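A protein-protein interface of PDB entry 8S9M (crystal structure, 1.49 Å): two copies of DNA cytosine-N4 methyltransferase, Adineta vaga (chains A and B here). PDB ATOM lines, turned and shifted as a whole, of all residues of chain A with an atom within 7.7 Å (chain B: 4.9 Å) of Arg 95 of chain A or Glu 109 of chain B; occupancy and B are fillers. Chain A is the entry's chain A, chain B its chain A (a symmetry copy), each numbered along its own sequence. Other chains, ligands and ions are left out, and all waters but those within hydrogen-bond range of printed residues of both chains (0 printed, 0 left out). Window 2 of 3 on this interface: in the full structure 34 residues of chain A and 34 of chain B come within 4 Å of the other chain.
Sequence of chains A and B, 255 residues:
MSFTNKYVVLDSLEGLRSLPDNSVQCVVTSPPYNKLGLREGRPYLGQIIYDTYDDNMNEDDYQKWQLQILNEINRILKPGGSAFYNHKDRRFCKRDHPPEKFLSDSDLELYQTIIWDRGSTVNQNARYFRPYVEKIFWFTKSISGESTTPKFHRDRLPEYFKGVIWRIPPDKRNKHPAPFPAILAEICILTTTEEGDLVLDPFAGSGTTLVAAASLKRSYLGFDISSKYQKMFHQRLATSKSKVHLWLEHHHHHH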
ATOM      1  N   LEU A  38       9.752 -10.977   7.865  1.00  0.00           N
ATOM      2  CA  LEU A  38       8.738  -9.928   7.950  1.00  0.00           C
ATOM      3  C   LEU A  38       8.632  -9.157   6.643  1.00  0.00           C
ATOM      4  O   LEU A  38       7.535  -8.737   6.254  1.00  0.00           O
ATOM      5  CB  LEU A  38       9.080  -8.979   9.098  1.00  0.00           C
ATOM      6  CG  LEU A  38       8.099  -7.845   9.408  1.00  0.00           C
ATOM      7  CD1 LEU A  38       6.731  -8.404   9.761  1.00  0.00           C
ATOM      8  CD2 LEU A  38       8.637  -6.997  10.538  1.00  0.00           C
ATOM      9  N   ASP A  89      11.151  -3.727  18.549  1.00  0.00           N
ATOM     10  CA  ASP A  89      10.139  -3.257  17.612  1.00  0.00           C
ATOM     11  C   ASP A  89      10.693  -3.315  16.193  1.00  0.00           C
ATOM     12  O   ASP A  89      11.809  -2.855  15.925  1.00  0.00           O
ATOM     13  CB  ASP A  89       9.749  -1.819  17.964  1.00  0.00           C
ATOM     14  CG  ASP A  89       8.937  -1.726  19.246  1.00  0.00           C
ATOM     15  OD1 ASP A  89       8.531  -2.782  19.777  1.00  0.00           O
ATOM     16  OD2 ASP A  89       8.705  -0.591  19.724  1.00  0.00           O
ATOM     17  N   ARG A  90       9.922  -3.904  15.290  1.00  0.00           N
ATOM     18  CA  ARG A  90      10.254  -3.977  13.875  1.00  0.00           C
ATOM     19  C   ARG A  90       9.325  -3.046  13.096  1.00  0.00           C
ATOM     20  O   ARG A  90       8.482  -2.353  13.674  1.00  0.00           O
ATOM     21  CB  ARG A  90      10.196  -5.429  13.393  1.00  0.00           C
ATOM     22  CG  ARG A  90      11.297  -6.309  14.001  1.00  0.00           C
ATOM     23  CD  ARG A  90      11.089  -7.774  13.683  1.00  0.00           C
ATOM     24  NE  ARG A  90       9.891  -8.274  14.337  1.00  0.00           N
ATOM     25  CZ  ARG A  90       9.194  -9.322  13.918  1.00  0.00           C
ATOM     26  NH1 ARG A  90       9.566 -10.019  12.853  1.00  0.00           N
ATOM     27  NH2 ARG A  90       8.105  -9.685  14.591  1.00  0.00           N
ATOM     28  N   ARG A  91       9.503  -3.006  11.777  1.00  0.00           N
ATOM     29  CA  ARG A  91       8.699  -2.159  10.902  1.00  0.00           C
ATOM     30  C   ARG A  91       7.968  -3.033   9.895  1.00  0.00           C
ATOM     31  O   ARG A  91       8.577  -3.911   9.277  1.00  0.00           O
ATOM     32  CB  ARG A  91       9.570  -1.165  10.125  1.00  0.00           C
ATOM     33  CG  ARG A  91      10.544  -0.341  10.942  1.00  0.00           C
ATOM     34  CD  ARG A  91       9.854   0.583  11.923  1.00  0.00           C
ATOM     35  NE  ARG A  91       8.956   1.545  11.292  1.00  0.00           N
ATOM     36  CZ  ARG A  91       8.254   2.450  11.961  1.00  0.00           C
ATOM     37  NH1 ARG A  91       8.377   2.591  13.272  1.00  0.00           N
ATOM     38  NH2 ARG A  91       7.406   3.231  11.302  1.00  0.00           N
ATOM     39  N   PHE A  92       6.671  -2.782   9.715  1.00  0.00           N
ATOM     40  CA  PHE A  92       5.891  -3.468   8.692  1.00  0.00           C
ATOM     41  C   PHE A  92       4.981  -2.455   8.020  1.00  0.00           C
ATOM     42  O   PHE A  92       4.141  -1.840   8.685  1.00  0.00           O
ATOM     43  CB  PHE A  92       5.059  -4.614   9.278  1.00  0.00           C
ATOM     44  CG  PHE A  92       4.273  -5.375   8.243  1.00  0.00           C
ATOM     45  CD1 PHE A  92       4.897  -6.303   7.425  1.00  0.00           C
ATOM     46  CD2 PHE A  92       2.914  -5.157   8.082  1.00  0.00           C
ATOM     47  CE1 PHE A  92       4.182  -7.000   6.469  1.00  0.00           C
ATOM     48  CE2 PHE A  92       2.192  -5.851   7.127  1.00  0.00           C
ATOM     49  CZ  PHE A  92       2.827  -6.773   6.319  1.00  0.00           C
ATOM     50  N   CYS A  93       5.148  -2.293   6.708  1.00  0.00           N
ATOM     51  CA  CYS A  93       4.316  -1.396   5.904  1.00  0.00           C
ATOM     52  C   CYS A  93       4.272   0.007   6.500  1.00  0.00           C
ATOM     53  O   CYS A  93       3.207   0.598   6.694  1.00  0.00           O
ATOM     54  CB  CYS A  93       2.913  -1.966   5.695  1.00  0.00           C
ATOM     55  SG  CYS A  93       2.864  -3.463   4.687  1.00  0.00           S
ATOM     56  N   LYS A  94       5.458   0.530   6.814  1.00  0.00           N
ATOM     57  CA  LYS A  94       5.638   1.880   7.343  1.00  0.00           C
ATOM     58  C   LYS A  94       4.942   2.091   8.685  1.00  0.00           C
ATOM     59  O   LYS A  94       4.654   3.228   9.065  1.00  0.00           O
ATOM     60  CB  LYS A  94       5.224   2.954   6.331  1.00  0.00           C
ATOM     61  CG  LYS A  94       5.840   2.777   4.954  1.00  0.00           C
ATOM     62  CD  LYS A  94       5.018   3.502   3.899  1.00  0.00           C
ATOM     63  CE  LYS A  94       3.547   3.112   3.997  1.00  0.00           C
ATOM     64  NZ  LYS A  94       2.714   3.705   2.913  1.00  0.00           N
ATOM     65  N   ARG A  95       4.659   1.018   9.419  1.00  0.00           N
ATOM     66  CA  ARG A  95       4.060   1.132  10.741  1.00  0.00           C
ATOM     67  C   ARG A  95       4.837   0.273  11.724  1.00  0.00           C
ATOM     68  O   ARG A  95       5.597  -0.617  11.335  1.00  0.00           O
ATOM     69  CB  ARG A  95       2.582   0.723  10.740  1.00  0.00           C
ATOM     70  CG  ARG A  95       1.692   1.607   9.867  1.00  0.00           C
ATOM     71  CD  ARG A  95       1.645   3.046  10.372  1.00  0.00           C
ATOM     72  NE  ARG A  95       0.809   3.892   9.525  1.00  0.00           N
ATOM     73  CZ  ARG A  95       1.273   4.676   8.561  1.00  0.00           C
ATOM     74  NH1 ARG A  95       2.566   4.760   8.300  1.00  0.00           N
ATOM     75  NH2 ARG A  95       0.415   5.396   7.840  1.00  0.00           N
ATOM     76  N   ASP A  96       4.635   0.561  13.011  1.00  0.00           N
ATOM     77  CA  ASP A  96       5.319  -0.163  14.071  1.00  0.00           C
ATOM     78  C   ASP A  96       4.839  -1.610  14.111  1.00  0.00           C
ATOM     79  O   ASP A  96       3.656  -1.894  13.913  1.00  0.00           O
ATOM     80  CB  ASP A  96       5.027   0.517  15.412  1.00  0.00           C
ATOM     81  CG  ASP A  96       5.903   0.004  16.540  1.00  0.00           C
ATOM     82  OD1 ASP A  96       7.134   0.201  16.475  1.00  0.00           O
ATOM     83  OD2 ASP A  96       5.360  -0.584  17.504  1.00  0.00           O
ATOM     84  N   HIS A  97       5.767  -2.532  14.364  1.00  0.00           N
ATOM     85  CA  HIS A  97       5.455  -3.959  14.477  1.00  0.00           C
ATOM     86  C   HIS A  97       6.109  -4.463  15.757  1.00  0.00           C
ATOM     87  O   HIS A  97       7.217  -5.011  15.727  1.00  0.00           O
ATOM     88  CB  HIS A  97       5.943  -4.716  13.238  1.00  0.00           C
ATOM     89  CG  HIS A  97       5.450  -6.128  13.141  1.00  0.00           C
ATOM     90  ND1 HIS A  97       4.168  -6.447  12.745  1.00  0.00           N
ATOM     91  CD2 HIS A  97       6.082  -7.307  13.350  1.00  0.00           C
ATOM     92  CE1 HIS A  97       4.026  -7.761  12.732  1.00  0.00           C
ATOM     93  NE2 HIS A  97       5.173  -8.307  13.096  1.00  0.00           N
ATOM     94  N   PRO A  98       5.455  -4.286  16.903  1.00  0.00           N
ATOM     95  CA  PRO A  98       6.106  -4.571  18.188  1.00  0.00           C
ATOM     96  C   PRO A  98       5.955  -6.030  18.577  1.00  0.00           C
ATOM     97  O   PRO A  98       5.007  -6.707  18.145  1.00  0.00           O
ATOM     98  CB  PRO A  98       5.341  -3.668  19.164  1.00  0.00           C
ATOM     99  CG  PRO A  98       3.975  -3.625  18.591  1.00  0.00           C
ATOM    100  CD  PRO A  98       4.154  -3.615  17.089  1.00  0.00           C
ATOM    101  N   LYS A 101       2.618  -7.700  20.120  1.00  0.00           N
ATOM    102  CA  LYS A 101       1.472  -8.179  19.358  1.00  0.00           C
ATOM    103  C   LYS A 101       1.345  -9.697  19.386  1.00  0.00           C
ATOM    104  O   LYS A 101       0.243 -10.213  19.178  1.00  0.00           O
ATOM    105  CB  LYS A 101       1.503  -7.655  17.924  1.00  0.00           C
ATOM    106  CG  LYS A 101       2.171  -8.575  16.930  1.00  0.00           C
ATOM    107  CD  LYS A 101       1.825  -8.151  15.515  1.00  0.00           C
ATOM    108  CE  LYS A 101       2.137  -6.681  15.316  1.00  0.00           C
ATOM    109  NZ  LYS A 101       3.562  -6.411  15.655  1.00  0.00           N
ATOM    110  N   ASP B 107      -8.564   2.607  16.292  1.00  0.00           N
ATOM    111  CA  ASP B 107      -8.462   2.855  14.857  1.00  0.00           C
ATOM    112  C   ASP B 107      -7.157   3.547  14.479  1.00  0.00           C
ATOM    113  O   ASP B 107      -6.761   3.501  13.307  1.00  0.00           O
ATOM    114  CB  ASP B 107      -9.620   3.740  14.393  1.00  0.00           C
ATOM    115  CG  ASP B 107     -10.982   3.121  14.653  1.00  0.00           C
ATOM    116  OD1 ASP B 107     -11.085   1.873  14.720  1.00  0.00           O
ATOM    117  OD2 ASP B 107     -11.961   3.893  14.775  1.00  0.00           O
ATOM    118  N   LEU B 108      -6.496   4.206  15.426  1.00  0.00           N
ATOM    119  CA  LEU B 108      -5.207   4.817  15.138  1.00  0.00           C
ATOM    120  C   LEU B 108      -4.179   3.742  14.829  1.00  0.00           C
ATOM    121  O   LEU B 108      -4.263   2.606  15.313  1.00  0.00           O
ATOM    122  CB  LEU B 108      -4.708   5.598  16.347  1.00  0.00           C
ATOM    123  CG  LEU B 108      -5.389   6.921  16.685  1.00  0.00           C
ATOM    124  CD1 LEU B 108      -4.949   7.407  18.055  1.00  0.00           C
ATOM    125  CD2 LEU B 108      -5.070   7.973  15.610  1.00  0.00           C
ATOM    126  N   GLU B 109      -3.187   4.109  14.024  1.00  0.00           N
ATOM    127  CA  GLU B 109      -2.092   3.204  13.690  1.00  0.00           C
ATOM    128  C   GLU B 109      -0.842   3.659  14.427  1.00  0.00           C
ATOM    129  O   GLU B 109      -0.418   4.809  14.288  1.00  0.00           O
ATOM    130  CB  GLU B 109      -1.863   3.156  12.180  1.00  0.00           C
ATOM    131  CG  GLU B 109      -2.984   2.434  11.441  1.00  0.00           C
ATOM    132  CD  GLU B 109      -2.770   2.378   9.941  1.00  0.00           C
ATOM    133  OE1 GLU B 109      -1.718   2.854   9.466  1.00  0.00           O
ATOM    134  OE2 GLU B 109      -3.660   1.854   9.238  1.00  0.00           O
ATOM    135  N   LEU B 110      -0.265   2.765  15.226  1.00  0.00           N
ATOM    136  CA  LEU B 110       0.941   3.112  15.965  1.00  0.00           C
ATOM    137  C   LEU B 110       2.115   3.218  15.004  1.00  0.00           C
ATOM    138  O   LEU B 110       2.405   2.279  14.253  1.00  0.00           O
ATOM    139  CB  LEU B 110       1.234   2.059  17.030  1.00  0.00           C
ATOM    140  CG  LEU B 110       2.449   2.358  17.901  1.00  0.00           C
ATOM    141  CD1 LEU B 110       2.255   3.643  18.692  1.00  0.00           C
ATOM    142  CD2 LEU B 110       2.689   1.189  18.836  1.00  0.00           C
ATOM    143  N   TYR B 111       2.776   4.373  15.014  1.00  0.00           N
ATOM    144  CA  TYR B 111       3.919   4.619  14.149  1.00  0.00           C
ATOM    145  C   TYR B 111       5.243   4.302  14.841  1.00  0.00           C
ATOM    146  O   TYR B 111       6.123   3.688  14.232  1.00  0.00           O
ATOM    147  CB  TYR B 111       3.882   6.066  13.635  1.00  0.00           C
ATOM    148  CG  TYR B 111       4.905   6.343  12.566  1.00  0.00           C
ATOM    149  CD1 TYR B 111       4.835   5.704  11.331  1.00  0.00           C
ATOM    150  CD2 TYR B 111       5.962   7.219  12.796  1.00  0.00           C
ATOM    151  CE1 TYR B 111       5.775   5.949  10.342  1.00  0.00           C
ATOM    152  CE2 TYR B 111       6.912   7.462  11.816  1.00  0.00           C
ATOM    153  CZ  TYR B 111       6.817   6.819  10.595  1.00  0.00           C
ATOM    154  OH  TYR B 111       7.767   7.054   9.621  1.00  0.00           O
ATOM    155  N   TRP B 138       3.443   7.375  19.435  1.00  0.00           N
ATOM    156  CA  TRP B 138       3.285   8.233  18.270  1.00  0.00           C
ATOM    157  C   TRP B 138       2.380   7.500  17.295  1.00  0.00           C
ATOM    158  O   TRP B 138       2.804   6.526  16.660  1.00  0.00           O
ATOM    159  CB  TRP B 138       4.656   8.513  17.669  1.00  0.00           C
ATOM    160  CG  TRP B 138       4.679   9.360  16.438  1.00  0.00           C
ATOM    161  CD1 TRP B 138       3.643  10.058  15.875  1.00  0.00           C
ATOM    162  CD2 TRP B 138       5.822   9.595  15.609  1.00  0.00           C
ATOM    163  NE1 TRP B 138       4.084  10.717  14.740  1.00  0.00           N
ATOM    164  CE2 TRP B 138       5.415  10.440  14.557  1.00  0.00           C
ATOM    165  CE3 TRP B 138       7.152   9.165  15.655  1.00  0.00           C
ATOM    166  CZ2 TRP B 138       6.294  10.869  13.565  1.00  0.00           C
ATOM    167  CZ3 TRP B 138       8.021   9.586  14.669  1.00  0.00           C
ATOM    168  CH2 TRP B 138       7.588  10.435  13.637  1.00  0.00           C
ATOM    169  N   PHE B 139       1.134   7.961  17.191  1.00  0.00           N
ATOM    170  CA  PHE B 139       0.141   7.385  16.301  1.00  0.00           C
ATOM    171  C   PHE B 139      -0.031   8.266  15.075  1.00  0.00           C
ATOM    172  O   PHE B 139       0.219   9.476  15.096  1.00  0.00           O
ATOM    173  CB  PHE B 139      -1.229   7.337  16.971  1.00  0.00           C
ATOM    174  CG  PHE B 139      -1.348   6.359  18.089  1.00  0.00           C
ATOM    175  CD1 PHE B 139      -1.512   5.007  17.830  1.00  0.00           C
ATOM    176  CD2 PHE B 139      -1.377   6.801  19.405  1.00  0.00           C
ATOM    177  CE1 PHE B 139      -1.671   4.105  18.870  1.00  0.00           C
ATOM    178  CE2 PHE B 139      -1.533   5.906  20.445  1.00  0.00           C
ATOM    179  CZ  PHE B 139      -1.682   4.555  20.179  1.00  0.00           C
ATOM    180  N   THR B 140      -0.523   7.654  14.011  1.00  0.00           N
ATOM    181  CA  THR B 140      -0.964   8.413  12.854  1.00  0.00           C
ATOM    182  C   THR B 140      -2.336   7.911  12.424  1.00  0.00           C
ATOM    183  O   THR B 140      -2.836   6.895  12.915  1.00  0.00           O
ATOM    184  CB  THR B 140       0.071   8.382  11.724  1.00  0.00           C
ATOM    185  OG1 THR B 140      -0.280   9.356  10.730  1.00  0.00           O
ATOM    186  CG2 THR B 140       0.144   7.017  11.096  1.00  0.00           C
ATOM    187  N   LYS B 141      -2.961   8.658  11.521  1.00  0.00           N
ATOM    188  CA  LYS B 141      -4.323   8.358  11.107  1.00  0.00           C
ATOM    189  C   LYS B 141      -4.360   7.107  10.234  1.00  0.00           C
ATOM    190  O   LYS B 141      -3.440   6.832   9.457  1.00  0.00           O
ATOM    191  CB  LYS B 141      -4.894   9.545  10.326  1.00  0.00           C
ATOM    192  CG  LYS B 141      -6.391   9.483  10.102  1.00  0.00           C
ATOM    193  CD  LYS B 141      -6.823  10.503   9.079  1.00  0.00           C
ATOM    194  CE  LYS B 141      -8.327  10.478   8.867  1.00  0.00           C
ATOM    195  NZ  LYS B 141      -9.074  11.163   9.967  1.00  0.00           N
ATOM    196  N   SER B 142      -5.440   6.346  10.359  1.00  0.00           N
ATOM    197  CA  SER B 142      -5.700   5.216   9.478  1.00  0.00           C
ATOM    198  C   SER B 142      -6.908   5.555   8.620  1.00  0.00           C
ATOM    199  O   SER B 142      -7.915   6.052   9.136  1.00  0.00           O
ATOM    200  CB  SER B 142      -6.005   3.957  10.283  1.00  0.00           C
ATOM    201  OG  SER B 142      -7.329   4.009  10.779  1.00  0.00           O
ATOM    202  N   THR B 149       3.668   7.802   5.336  1.00  0.00           N
ATOM    203  CA  THR B 149       4.255   8.209   6.608  1.00  0.00           C
ATOM    204  C   THR B 149       3.766   9.597   7.026  1.00  0.00           C
ATOM    205  O   THR B 149       3.472  10.439   6.175  1.00  0.00           O
ATOM    206  CB  THR B 149       5.798   8.214   6.544  1.00  0.00           C
ATOM    207  OG1 THR B 149       6.232   9.098   5.503  1.00  0.00           O
ATOM    208  CG2 THR B 149       6.330   6.813   6.268  1.00  0.00           C
ATOM    209  N   PRO B 150       3.679   9.833   8.334  1.00  0.00           N
ATOM    210  CA  PRO B 150       3.259  11.152   8.818  1.00  0.00           C
ATOM    211  C   PRO B 150       4.275  12.231   8.479  1.00  0.00           C
ATOM    212  O   PRO B 150       5.465  11.967   8.290  1.00  0.00           O
ATOM    213  CB  PRO B 150       3.165  10.959  10.339  1.00  0.00           C
ATOM    214  CG  PRO B 150       4.022   9.765  10.630  1.00  0.00           C
ATOM    215  CD  PRO B 150       3.898   8.879   9.435  1.00  0.00           C
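O of Tyr 111 of chain B lies within hydrogen-bond range of NH1 of Arg 91 of chain A (2.7 Å).
The backbone NH of Asp 96 of chain A sits at hydrogen-bond distance from the backbone carbonyl oxygen of Leu 110 of chain B.
The side-chain carboxylate (OE1) of Glu 109 of chain B lies within salt-bridge range of the guanidinium group (NE) of Arg 95 of chain A (2.7 Å).
O of Trp 138 of chain B lies within hydrogen-bond range of N of Tyr 111 of chain B (2.7 Å).
The backbone carbonyl oxygen (O) of Glu 109 of chain B sits at hydrogen-bond distance from the backbone NH (N) of Thr 140 of chain B.
Tyr 111 of chain B touches Lys 94 of chain A.
CB of Arg 95 of chain A touches O of Leu 110 of chain B, at 3.8 Å.
Arg 95 of chain A touches Tyr 111 of chain B (NH1 to CD1, 3.9 Å).
Thr 140 of chain B touches Arg 95 of chain A.
Tyr 111 of chain B touches Asp 96 of chain A.
Leu 38 of chain A touches none of the printed residues of chain B.
Arg 95 of chain A touches just these residues of chain B: Glu 109, Leu 110, Tyr 111 and Thr 140.
Printed residues of chain B within 4 Å of Asp 96 of chain A: Leu 110 (3.1 Å) and Tyr 111 (3.6 Å).
Of the printed residues of chain A, Thr 140 of chain B touches Arg 95.
The nearest residue of chain B that does not touch Arg 95 of chain A is Thr 149 of chain B (4.2 Å).
The nearest residue of chain A that does not touch Glu 109 of chain B is Cys 93 of chain A (6.1 Å).
Hydrophobic or aromatic side chains of chain B that line the printed part of chain A: Leu 110 and Tyr 111.
Among the printed residues, Asp or Glu carboxylates within 4 Å of a Lys or Arg side-chain nitrogen of the other chain: Arg 95 of chain A with Glu 109 of chain B.
No position is printed for both chains.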
